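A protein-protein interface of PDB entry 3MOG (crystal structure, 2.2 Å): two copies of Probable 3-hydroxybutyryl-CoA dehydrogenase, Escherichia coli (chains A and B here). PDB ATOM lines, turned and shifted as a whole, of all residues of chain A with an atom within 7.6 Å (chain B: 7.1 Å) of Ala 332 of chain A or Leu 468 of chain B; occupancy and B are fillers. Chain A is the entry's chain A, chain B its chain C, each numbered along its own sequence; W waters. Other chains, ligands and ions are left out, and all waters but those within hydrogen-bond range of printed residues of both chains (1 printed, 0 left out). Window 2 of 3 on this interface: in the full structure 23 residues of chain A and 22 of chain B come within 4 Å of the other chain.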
ATOM      1  N   GLY A 327     -26.362  29.001   1.983  1.00  0.00           N
ATOM      2  CA  GLY A 327     -25.511  27.827   2.157  1.00  0.00           C
ATOM      3  C   GLY A 327     -24.264  27.758   1.315  1.00  0.00           C
ATOM      4  O   GLY A 327     -23.469  26.825   1.460  1.00  0.00           O
ATOM      5  N   GLU A 328     -24.104  28.733   0.427  1.00  0.00           N
ATOM      6  CA  GLU A 328     -22.934  28.833  -0.435  1.00  0.00           C
ATOM      7  C   GLU A 328     -22.010  29.889   0.123  1.00  0.00           C
ATOM      8  O   GLU A 328     -22.473  30.862   0.705  1.00  0.00           O
ATOM      9  CB  GLU A 328     -23.358  29.219  -1.842  1.00  0.00           C
ATOM     10  CG  GLU A 328     -24.039  28.114  -2.623  1.00  0.00           C
ATOM     11  CD  GLU A 328     -24.395  28.538  -4.035  1.00  0.00           C
ATOM     12  OE1 GLU A 328     -24.206  27.723  -4.962  1.00  0.00           O
ATOM     13  OE2 GLU A 328     -24.857  29.684  -4.224  1.00  0.00           O
ATOM     14  N   THR A 329     -20.703  29.706  -0.044  1.00  0.00           N
ATOM     15  CA  THR A 329     -19.753  30.651   0.544  1.00  0.00           C
ATOM     16  C   THR A 329     -19.708  31.957  -0.242  1.00  0.00           C
ATOM     17  O   THR A 329     -19.971  31.971  -1.452  1.00  0.00           O
ATOM     18  CB  THR A 329     -18.340  30.076   0.623  1.00  0.00           C
ATOM     19  OG1 THR A 329     -17.906  29.717  -0.689  1.00  0.00           O
ATOM     20  CG2 THR A 329     -18.310  28.855   1.523  1.00  0.00           C
ATOM     21  N   ALA A 330     -19.367  33.042   0.454  1.00  0.00           N
ATOM     22  CA  ALA A 330     -19.133  34.342  -0.180  1.00  0.00           C
ATOM     23  C   ALA A 330     -18.160  34.231  -1.348  1.00  0.00           C
ATOM     24  O   ALA A 330     -18.393  34.807  -2.401  1.00  0.00           O
ATOM     25  CB  ALA A 330     -18.631  35.364   0.844  1.00  0.00           C
ATOM     26  N   GLN A 331     -17.090  33.471  -1.150  1.00  0.00           N
ATOM     27  CA  GLN A 331     -16.101  33.222  -2.180  1.00  0.00           C
ATOM     28  C   GLN A 331     -16.659  32.516  -3.427  1.00  0.00           C
ATOM     29  O   GLN A 331     -16.256  32.837  -4.560  1.00  0.00           O
ATOM     30  CB  GLN A 331     -14.925  32.434  -1.584  1.00  0.00           C
ATOM     31  CG  GLN A 331     -13.794  32.073  -2.556  1.00  0.00           C
ATOM     32  CD  GLN A 331     -12.935  33.261  -3.018  1.00  0.00           C
ATOM     33  OE1 GLN A 331     -13.095  34.409  -2.575  1.00  0.00           O
ATOM     34  NE2 GLN A 331     -12.010  32.973  -3.928  1.00  0.00           N
ATOM     35  N   ALA A 332     -17.580  31.570  -3.222  1.00  0.00           N
ATOM     36  CA  ALA A 332     -18.115  30.777  -4.330  1.00  0.00           C
ATOM     37  C   ALA A 332     -18.961  31.645  -5.241  1.00  0.00           C
ATOM     38  O   ALA A 332     -18.912  31.514  -6.472  1.00  0.00           O
ATOM     39  CB  ALA A 332     -18.929  29.626  -3.814  1.00  0.00           C
ATOM     40  N   LEU A 333     -19.721  32.528  -4.604  1.00  0.00           N
ATOM     41  CA  LEU A 333     -20.572  33.490  -5.262  1.00  0.00           C
ATOM     42  C   LEU A 333     -19.695  34.519  -5.969  1.00  0.00           C
ATOM     43  O   LEU A 333     -19.857  34.756  -7.170  1.00  0.00           O
ATOM     44  CB  LEU A 333     -21.485  34.153  -4.228  1.00  0.00           C
ATOM     45  CG  LEU A 333     -22.569  33.248  -3.619  1.00  0.00           C
ATOM     46  CD1 LEU A 333     -23.142  33.860  -2.369  1.00  0.00           C
ATOM     47  CD2 LEU A 333     -23.677  32.971  -4.624  1.00  0.00           C
ATOM     48  N   ALA A 334     -18.733  35.075  -5.229  1.00  0.00           N
ATOM     49  CA  ALA A 334     -17.810  36.071  -5.762  1.00  0.00           C
ATOM     50  C   ALA A 334     -17.214  35.688  -7.108  1.00  0.00           C
ATOM     51  O   ALA A 334     -17.259  36.484  -8.038  1.00  0.00           O
ATOM     52  CB  ALA A 334     -16.714  36.394  -4.768  1.00  0.00           C
ATOM     53  N   ILE A 335     -16.691  34.474  -7.231  1.00  0.00           N
ATOM     54  CA  ILE A 335     -16.114  34.078  -8.509  1.00  0.00           C
ATOM     55  C   ILE A 335     -17.147  33.650  -9.561  1.00  0.00           C
ATOM     56  O   ILE A 335     -16.844  33.643 -10.755  1.00  0.00           O
ATOM     57  CB  ILE A 335     -14.939  33.047  -8.392  1.00  0.00           C
ATOM     58  CG1 ILE A 335     -15.447  31.606  -8.428  1.00  0.00           C
ATOM     59  CG2 ILE A 335     -14.017  33.366  -7.187  1.00  0.00           C
ATOM     60  CD1 ILE A 335     -14.635  30.713  -9.363  1.00  0.00           C
ATOM     61  N   ARG A 336     -18.358  33.305  -9.128  1.00  0.00           N
ATOM     62  CA  ARG A 336     -19.400  32.914 -10.082  1.00  0.00           C
ATOM     63  C   ARG A 336     -20.211  34.110 -10.570  1.00  0.00           C
ATOM     64  O   ARG A 336     -20.786  34.073 -11.657  1.00  0.00           O
ATOM     65  CB  ARG A 336     -20.328  31.852  -9.496  1.00  0.00           C
ATOM     66  CG  ARG A 336     -21.024  30.989 -10.552  1.00  0.00           C
ATOM     67  CD  ARG A 336     -21.788  29.852  -9.909  1.00  0.00           C
ATOM     68  NE  ARG A 336     -22.765  30.355  -8.947  1.00  0.00           N
ATOM     69  CZ  ARG A 336     -23.147  29.708  -7.851  1.00  0.00           C
ATOM     70  NH1 ARG A 336     -22.632  28.515  -7.559  1.00  0.00           N
ATOM     71  NH2 ARG A 336     -24.044  30.258  -7.042  1.00  0.00           N
ATOM     72  N   LEU A 337     -20.259  35.165  -9.767  1.00  0.00           N
ATOM     73  CA  LEU A 337     -20.928  36.387 -10.181  1.00  0.00           C
ATOM     74  C   LEU A 337     -19.920  37.436 -10.677  1.00  0.00           C
ATOM     75  O   LEU A 337     -20.314  38.511 -11.132  1.00  0.00           O
ATOM     76  CB  LEU A 337     -21.835  36.930  -9.065  1.00  0.00           C
ATOM     77  CG  LEU A 337     -22.932  35.992  -8.518  1.00  0.00           C
ATOM     78  CD1 LEU A 337     -23.949  36.770  -7.691  1.00  0.00           C
ATOM     79  CD2 LEU A 337     -23.648  35.196  -9.611  1.00  0.00           C
ATOM     80  N   ALA A 338     -18.631  37.079 -10.599  1.00  0.00           N
ATOM     81  CA  ALA A 338     -17.476  37.906 -11.005  1.00  0.00           C
ATOM     82  C   ALA A 338     -17.441  39.287 -10.359  1.00  0.00           C
ATOM     83  O   ALA A 338     -16.977  40.252 -10.958  1.00  0.00           O
ATOM     84  CB  ALA A 338     -17.368  38.002 -12.538  1.00  0.00           C
ATOM     85  N   VAL A 341     -18.499  39.927  -3.100  1.00  0.00           N
ATOM     86  CA  VAL A 341     -19.657  39.446  -2.336  1.00  0.00           C
ATOM     87  C   VAL A 341     -19.397  39.499  -0.828  1.00  0.00           C
ATOM     88  O   VAL A 341     -18.341  39.072  -0.353  1.00  0.00           O
ATOM     89  CB  VAL A 341     -20.111  38.020  -2.793  1.00  0.00           C
ATOM     90  CG1 VAL A 341     -21.113  37.394  -1.814  1.00  0.00           C
ATOM     91  CG2 VAL A 341     -20.733  38.074  -4.169  1.00  0.00           C
ATOM     92  N   VAL A 343     -21.488  38.046   2.414  1.00  0.00           N
ATOM     93  CA  VAL A 343     -22.608  37.195   2.815  1.00  0.00           C
ATOM     94  C   VAL A 343     -23.103  37.657   4.169  1.00  0.00           C
ATOM     95  O   VAL A 343     -22.301  38.008   5.031  1.00  0.00           O
ATOM     96  CB  VAL A 343     -22.230  35.687   2.784  1.00  0.00           C
ATOM     97  CG1 VAL A 343     -23.056  34.864   3.766  1.00  0.00           C
ATOM     98  CG2 VAL A 343     -22.376  35.144   1.363  1.00  0.00           C
ATOM     99  N   ALA A 357     -15.815  37.622   1.095  1.00  0.00           N
ATOM    100  CA  ALA A 357     -15.108  36.750   0.175  1.00  0.00           C
ATOM    101  C   ALA A 357     -13.645  37.199   0.137  1.00  0.00           C
ATOM    102  O   ALA A 357     -13.370  38.400   0.159  1.00  0.00           O
ATOM    103  CB  ALA A 357     -15.718  36.829  -1.187  1.00  0.00           C
ATOM    104  N   ALA A 358     -12.724  36.232   0.084  1.00  0.00           N
ATOM    105  CA  ALA A 358     -11.276  36.496   0.106  1.00  0.00           C
ATOM    106  C   ALA A 358     -10.798  37.387  -1.051  1.00  0.00           C
ATOM    107  O   ALA A 358      -9.847  38.155  -0.907  1.00  0.00           O
ATOM    108  CB  ALA A 358     -10.498  35.174   0.122  1.00  0.00           C
ATOM    109  N   ASP A 384     -15.816  32.790   6.345  1.00  0.00           N
ATOM    110  CA  ASP A 384     -16.676  32.498   5.221  1.00  0.00           C
ATOM    111  C   ASP A 384     -17.191  31.047   5.336  1.00  0.00           C
ATOM    112  O   ASP A 384     -16.693  30.134   4.674  1.00  0.00           O
ATOM    113  CB  ASP A 384     -15.919  32.735   3.915  1.00  0.00           C
ATOM    114  CG  ASP A 384     -16.826  32.732   2.714  1.00  0.00           C
ATOM    115  OD1 ASP A 384     -18.066  32.766   2.901  1.00  0.00           O
ATOM    116  OD2 ASP A 384     -16.294  32.699   1.581  1.00  0.00           O
ATOM    117  N   HIS A 451     -22.041  20.811  -0.202  1.00  0.00           N
ATOM    118  CA  HIS A 451     -20.751  21.335   0.247  1.00  0.00           C
ATOM    119  C   HIS A 451     -19.989  20.346   1.139  1.00  0.00           C
ATOM    120  O   HIS A 451     -18.788  20.109   0.938  1.00  0.00           O
ATOM    121  CB  HIS A 451     -20.919  22.662   1.004  1.00  0.00           C
ATOM    122  CG  HIS A 451     -19.617  23.294   1.381  1.00  0.00           C
ATOM    123  ND1 HIS A 451     -18.984  24.225   0.582  1.00  0.00           N
ATOM    124  CD2 HIS A 451     -18.804  23.104   2.448  1.00  0.00           C
ATOM    125  CE1 HIS A 451     -17.840  24.581   1.141  1.00  0.00           C
ATOM    126  NE2 HIS A 451     -17.714  23.925   2.281  1.00  0.00           N
ATOM    127  N   TRP B 438      -5.304  21.595  -6.994  1.00  0.00           N
ATOM    128  CA  TRP B 438      -6.506  21.464  -6.162  1.00  0.00           C
ATOM    129  C   TRP B 438      -7.809  21.139  -6.900  1.00  0.00           C
ATOM    130  O   TRP B 438      -8.619  20.347  -6.412  1.00  0.00           O
ATOM    131  CB  TRP B 438      -6.679  22.704  -5.278  1.00  0.00           C
ATOM    132  CG  TRP B 438      -5.487  22.961  -4.383  1.00  0.00           C
ATOM    133  CD1 TRP B 438      -4.606  24.013  -4.467  1.00  0.00           C
ATOM    134  CD2 TRP B 438      -5.024  22.144  -3.292  1.00  0.00           C
ATOM    135  NE1 TRP B 438      -3.641  23.903  -3.495  1.00  0.00           N
ATOM    136  CE2 TRP B 438      -3.878  22.780  -2.751  1.00  0.00           C
ATOM    137  CE3 TRP B 438      -5.471  20.951  -2.710  1.00  0.00           C
ATOM    138  CZ2 TRP B 438      -3.177  22.260  -1.658  1.00  0.00           C
ATOM    139  CZ3 TRP B 438      -4.770  20.437  -1.625  1.00  0.00           C
ATOM    140  CH2 TRP B 438      -3.631  21.090  -1.118  1.00  0.00           C
ATOM    141  N   GLN B 439      -7.998  21.726  -8.082  1.00  0.00           N
ATOM    142  CA  GLN B 439      -9.189  21.464  -8.870  1.00  0.00           C
ATOM    143  C   GLN B 439      -9.185  20.047  -9.400  1.00  0.00           C
ATOM    144  O   GLN B 439     -10.237  19.420  -9.513  1.00  0.00           O
ATOM    145  CB  GLN B 439      -9.307  22.439 -10.034  1.00  0.00           C
ATOM    146  CG  GLN B 439      -9.670  23.835  -9.623  1.00  0.00           C
ATOM    147  CD  GLN B 439      -9.442  24.813 -10.745  1.00  0.00           C
ATOM    148  OE1 GLN B 439     -10.379  25.193 -11.439  1.00  0.00           O
ATOM    149  NE2 GLN B 439      -8.186  25.201 -10.953  1.00  0.00           N
ATOM    150  N   LEU B 442      -9.992  17.773  -6.449  1.00  0.00           N
ATOM    151  CA  LEU B 442     -11.427  17.970  -6.233  1.00  0.00           C
ATOM    152  C   LEU B 442     -12.297  17.202  -7.222  1.00  0.00           C
ATOM    153  O   LEU B 442     -13.213  16.500  -6.809  1.00  0.00           O
ATOM    154  CB  LEU B 442     -11.795  19.460  -6.268  1.00  0.00           C
ATOM    155  CG  LEU B 442     -13.270  19.788  -6.190  1.00  0.00           C
ATOM    156  CD1 LEU B 442     -13.798  19.563  -4.761  1.00  0.00           C
ATOM    157  CD2 LEU B 442     -13.552  21.195  -6.682  1.00  0.00           C
ATOM    158  N   LEU B 462     -12.308  22.531   3.036  1.00  0.00           N
ATOM    159  CA  LEU B 462     -11.064  23.248   2.664  1.00  0.00           C
ATOM    160  C   LEU B 462     -10.547  22.897   1.265  1.00  0.00           C
ATOM    161  O   LEU B 462      -9.909  23.729   0.607  1.00  0.00           O
ATOM    162  CB  LEU B 462      -9.955  23.037   3.717  1.00  0.00           C
ATOM    163  CG  LEU B 462      -8.654  23.843   3.569  1.00  0.00           C
ATOM    164  CD1 LEU B 462      -8.933  25.354   3.610  1.00  0.00           C
ATOM    165  CD2 LEU B 462      -7.648  23.453   4.650  1.00  0.00           C
ATOM    166  N   LEU B 463     -10.807  21.672   0.810  1.00  0.00           N
ATOM    167  CA  LEU B 463     -10.482  21.315  -0.560  1.00  0.00           C
ATOM    168  C   LEU B 463     -11.302  22.139  -1.540  1.00  0.00           C
ATOM    169  O   LEU B 463     -10.718  22.728  -2.460  1.00  0.00           O
ATOM    170  CB  LEU B 463     -10.614  19.809  -0.837  1.00  0.00           C
ATOM    171  CG  LEU B 463     -10.333  19.281  -2.254  1.00  0.00           C
ATOM    172  CD1 LEU B 463      -8.934  19.595  -2.765  1.00  0.00           C
ATOM    173  CD2 LEU B 463     -10.568  17.780  -2.325  1.00  0.00           C
ATOM    174  N   ARG B 464     -12.623  22.214  -1.346  1.00  0.00           N
ATOM    175  CA  ARG B 464     -13.461  23.083  -2.215  1.00  0.00           C
ATOM    176  C   ARG B 464     -12.957  24.523  -2.177  1.00  0.00           C
ATOM    177  O   ARG B 464     -12.857  25.178  -3.216  1.00  0.00           O
ATOM    178  CB  ARG B 464     -14.956  23.066  -1.842  1.00  0.00           C
ATOM    179  CG  ARG B 464     -15.587  21.662  -1.766  1.00  0.00           C
ATOM    180  CD  ARG B 464     -17.114  21.738  -1.742  1.00  0.00           C
ATOM    181  NE  ARG B 464     -17.705  20.408  -1.786  1.00  0.00           N
ATOM    182  CZ  ARG B 464     -17.960  19.720  -2.895  1.00  0.00           C
ATOM    183  NH1 ARG B 464     -17.702  20.230  -4.097  1.00  0.00           N
ATOM    184  NH2 ARG B 464     -18.502  18.515  -2.801  1.00  0.00           N
ATOM    185  N   GLN B 465     -12.635  24.986  -0.968  1.00  0.00           N
ATOM    186  CA  GLN B 465     -12.108  26.320  -0.722  1.00  0.00           C
ATOM    187  C   GLN B 465     -10.814  26.559  -1.491  1.00  0.00           C
ATOM    188  O   GLN B 465     -10.644  27.620  -2.099  1.00  0.00           O
ATOM    189  CB  GLN B 465     -11.905  26.527   0.782  1.00  0.00           C
ATOM    190  CG  GLN B 465     -11.297  27.865   1.230  1.00  0.00           C
ATOM    191  CD  GLN B 465     -11.322  28.040   2.765  1.00  0.00           C
ATOM    192  OE1 GLN B 465     -10.424  28.668   3.352  1.00  0.00           O
ATOM    193  NE2 GLN B 465     -12.350  27.474   3.416  1.00  0.00           N
ATOM    194  N   ARG B 466      -9.920  25.572  -1.492  1.00  0.00           N
ATOM    195  CA  ARG B 466      -8.651  25.725  -2.208  1.00  0.00           C
ATOM    196  C   ARG B 466      -8.764  25.582  -3.726  1.00  0.00           C
ATOM    197  O   ARG B 466      -7.988  26.200  -4.463  1.00  0.00           O
ATOM    198  CB  ARG B 466      -7.561  24.817  -1.640  1.00  0.00           C
ATOM    199  CG  ARG B 466      -7.036  25.335  -0.313  1.00  0.00           C
ATOM    200  CD  ARG B 466      -5.694  24.745   0.014  1.00  0.00           C
ATOM    201  NE  ARG B 466      -5.197  25.313   1.253  1.00  0.00           N
ATOM    202  CZ  ARG B 466      -4.076  24.958   1.871  1.00  0.00           C
ATOM    203  NH1 ARG B 466      -3.293  24.000   1.381  1.00  0.00           N
ATOM    204  NH2 ARG B 466      -3.745  25.567   3.000  1.00  0.00           N
ATOM    205  N   ALA B 467      -9.735  24.790  -4.184  1.00  0.00           N
ATOM    206  CA  ALA B 467     -10.012  24.655  -5.609  1.00  0.00           C
ATOM    207  C   ALA B 467     -10.546  25.964  -6.169  1.00  0.00           C
ATOM    208  O   ALA B 467     -10.123  26.397  -7.242  1.00  0.00           O
ATOM    209  CB  ALA B 467     -10.997  23.540  -5.865  1.00  0.00           C
ATOM    210  N   LEU B 468     -11.460  26.585  -5.427  1.00  0.00           N
ATOM    211  CA  LEU B 468     -11.993  27.905  -5.769  1.00  0.00           C
ATOM    212  C   LEU B 468     -10.933  28.999  -5.849  1.00  0.00           C
ATOM    213  O   LEU B 468     -11.008  29.838  -6.740  1.00  0.00           O
ATOM    214  CB  LEU B 468     -13.106  28.323  -4.809  1.00  0.00           C
ATOM    215  CG  LEU B 468     -14.481  27.758  -5.163  1.00  0.00           C
ATOM    216  CD1 LEU B 468     -15.427  27.785  -3.978  1.00  0.00           C
ATOM    217  CD2 LEU B 468     -15.086  28.512  -6.348  1.00  0.00           C
ATOM    218  N   LEU B 469      -9.959  28.983  -4.938  1.00  0.00           N
ATOM    219  CA  LEU B 469      -8.876  29.973  -4.956  1.00  0.00           C
ATOM    220  C   LEU B 469      -7.974  29.759  -6.168  1.00  0.00           C
ATOM    221  O   LEU B 469      -7.589  30.724  -6.832  1.00  0.00           O
ATOM    222  CB  LEU B 469      -8.065  29.966  -3.649  1.00  0.00           C
ATOM    223  CG  LEU B 469      -8.755  30.511  -2.381  1.00  0.00           C
ATOM    224  CD1 LEU B 469      -8.155  29.912  -1.097  1.00  0.00           C
ATOM    225  CD2 LEU B 469      -8.709  32.049  -2.333  1.00  0.00           C
ATOM    226  N   GLU B 470      -7.689  28.491  -6.468  1.00  0.00           N
ATOM    227  CA  GLU B 470      -6.863  28.105  -7.610  1.00  0.00           C
ATOM    228  C   GLU B 470      -7.480  28.486  -8.963  1.00  0.00           C
ATOM    229  O   GLU B 470      -6.755  28.830  -9.899  1.00  0.00           O
ATOM    230  CB  GLU B 470      -6.571  26.612  -7.570  1.00  0.00           C
ATOM    231  CG  GLU B 470      -5.420  26.157  -8.455  1.00  0.00           C
ATOM    232  CD  GLU B 470      -5.303  24.656  -8.505  1.00  0.00           C
ATOM    233  OE1 GLU B 470      -6.191  24.007  -9.113  1.00  0.00           O
ATOM    234  OE2 GLU B 470      -4.322  24.126  -7.931  1.00  0.00           O
ATOM    235  N   SER B 471      -8.804  28.433  -9.067  1.00  0.00           N
ATOM    236  CA  SER B 471      -9.490  28.918 -10.266  1.00  0.00           C
ATOM    237  C   SER B 471      -9.466  30.453 -10.358  1.00  0.00           C
ATOM    238  O   SER B 471      -9.529  31.004 -11.456  1.00  0.00           O
ATOM    239  CB  SER B 471     -10.923  28.369 -10.375  1.00  0.00           C
ATOM    240  OG  SER B 471     -11.769  28.918  -9.384  1.00  0.00           O
ATOM    241  N   GLY B 472      -9.355  31.127  -9.211  1.00  0.00           N
ATOM    242  CA  GLY B 472      -9.164  32.584  -9.155  1.00  0.00           C
ATOM    243  C   GLY B 472      -7.883  33.095  -9.803  1.00  0.00           C
ATOM    244  O   GLY B 472      -7.881  34.173 -10.404  1.00  0.00           O
ATOM    245  N   TYR B 473      -6.796  32.327  -9.685  1.00  0.00           N
ATOM    246  CA  TYR B 473      -5.521  32.657 -10.344  1.00  0.00           C
ATOM    247  C   TYR B 473      -5.484  32.219 -11.814  1.00  0.00           C
ATOM    248  O   TYR B 473      -4.614  32.659 -12.570  1.00  0.00           O
ATOM    249  CB  TYR B 473      -4.317  32.040  -9.608  1.00  0.00           C
ATOM    250  CG  TYR B 473      -4.214  32.358  -8.127  1.00  0.00           C
ATOM    251  CD1 TYR B 473      -3.961  33.660  -7.678  1.00  0.00           C
ATOM    252  CD2 TYR B 473      -4.342  31.346  -7.172  1.00  0.00           C
ATOM    253  CE1 TYR B 473      -3.863  33.945  -6.313  1.00  0.00           C
ATOM    254  CE2 TYR B 473      -4.245  31.619  -5.809  1.00  0.00           C
ATOM    255  CZ  TYR B 473      -4.005  32.918  -5.389  1.00  0.00           C
ATOM    256  OH  TYR B 473      -3.908  33.179  -4.043  1.00  0.00           O
HETATM  257  O   HOH W   1     -18.139  17.448  -0.029  1.00  0.00           O
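Ala 332 of chain A touches just one residue of chain B: Leu 468.
No residue of chain A comes within 4 Å of Ala 467 of chain B.
Printed residues of chain A within 4 Å of Ser 471 of chain B: Ile 335.
Of the printed residues of chain A, Arg 464 of chain B touches His 451 (2.9 Å).
Of the printed residues of chain B, Ile 335 of chain A touches Leu 468 and Ser 471.
Printed residues of chain A within 4 Å of Leu 469 of chain B: Gln 331.
Of the printed residues of chain B, His 451 of chain A touches Arg 464.
Tyr 473 of chain B touches none of the printed residues of chain A.
Val 343 of chain A touches none of the printed residues of chain B.
The nearest printed residue of chain B that does not touch Ala 332 of chain A is Arg 464 of chain B (7.6 Å).
The nearest residue of chain A that does not touch Leu 468 of chain B is Gln 331 of chain A (4.3 Å).
The nearest printed residue of chain B that does not touch Gln 331 of chain A is Leu 468 of chain B (4.3 Å).
Water W1 lies within hydrogen-bond range of the backbone carbonyl oxygen (O) of His 451 of chain A and the guanidinium group (NH2) of Arg 464 of chain B.
Hydrophobic or aromatic side chains of chain B within 4 Å of the printed part of chain A: Leu 468 and Leu 469.
Hydrophobic or aromatic side chains of chain A that line the printed part of chain B: Ala 332, Ile 335 and His 451.
Among the printed residues, no Asp or Glu carboxylate lies within 4 Å of a Lys or Arg side-chain nitrogen of the other chain.
The backbone carbonyl oxygen of His 451 of chain A is in hydrogen-bond range of the guanidinium group of Arg 464 of chain B.
No position is printed for both chains.
Among the printed residues, pairs that only touch across the chains: Gln 331 of chain A with Leu 469 of chain B, Ala 332 of chain A with Leu 468 of chain B, Ile 335 of chain A with Leu 468 of chain B and Ile 335 of chain A with Ser 471 of chain B.
The side-chain amide oxygen (OE1) of Gln 331 of chain A sits at hydrogen-bond distance from the backbone NH (N) of Ala 358 of chain A (3.2 Å).
N of Gln 331 of chain A is in hydrogen-bond range of OD2 of Asp 384 of chain A, 2.9 Å away.
The side-chain hydroxyl of Thr 329 of chain A is in hydrogen-bond range of the backbone NH of Ala 332 of chain A (3.2 Å).
The backbone carbonyl oxygen (O) of Leu 468 of chain B sits at hydrogen-bond distance from the side-chain hydroxyl (OG) of Ser 471 of chain B (2.9 Å).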
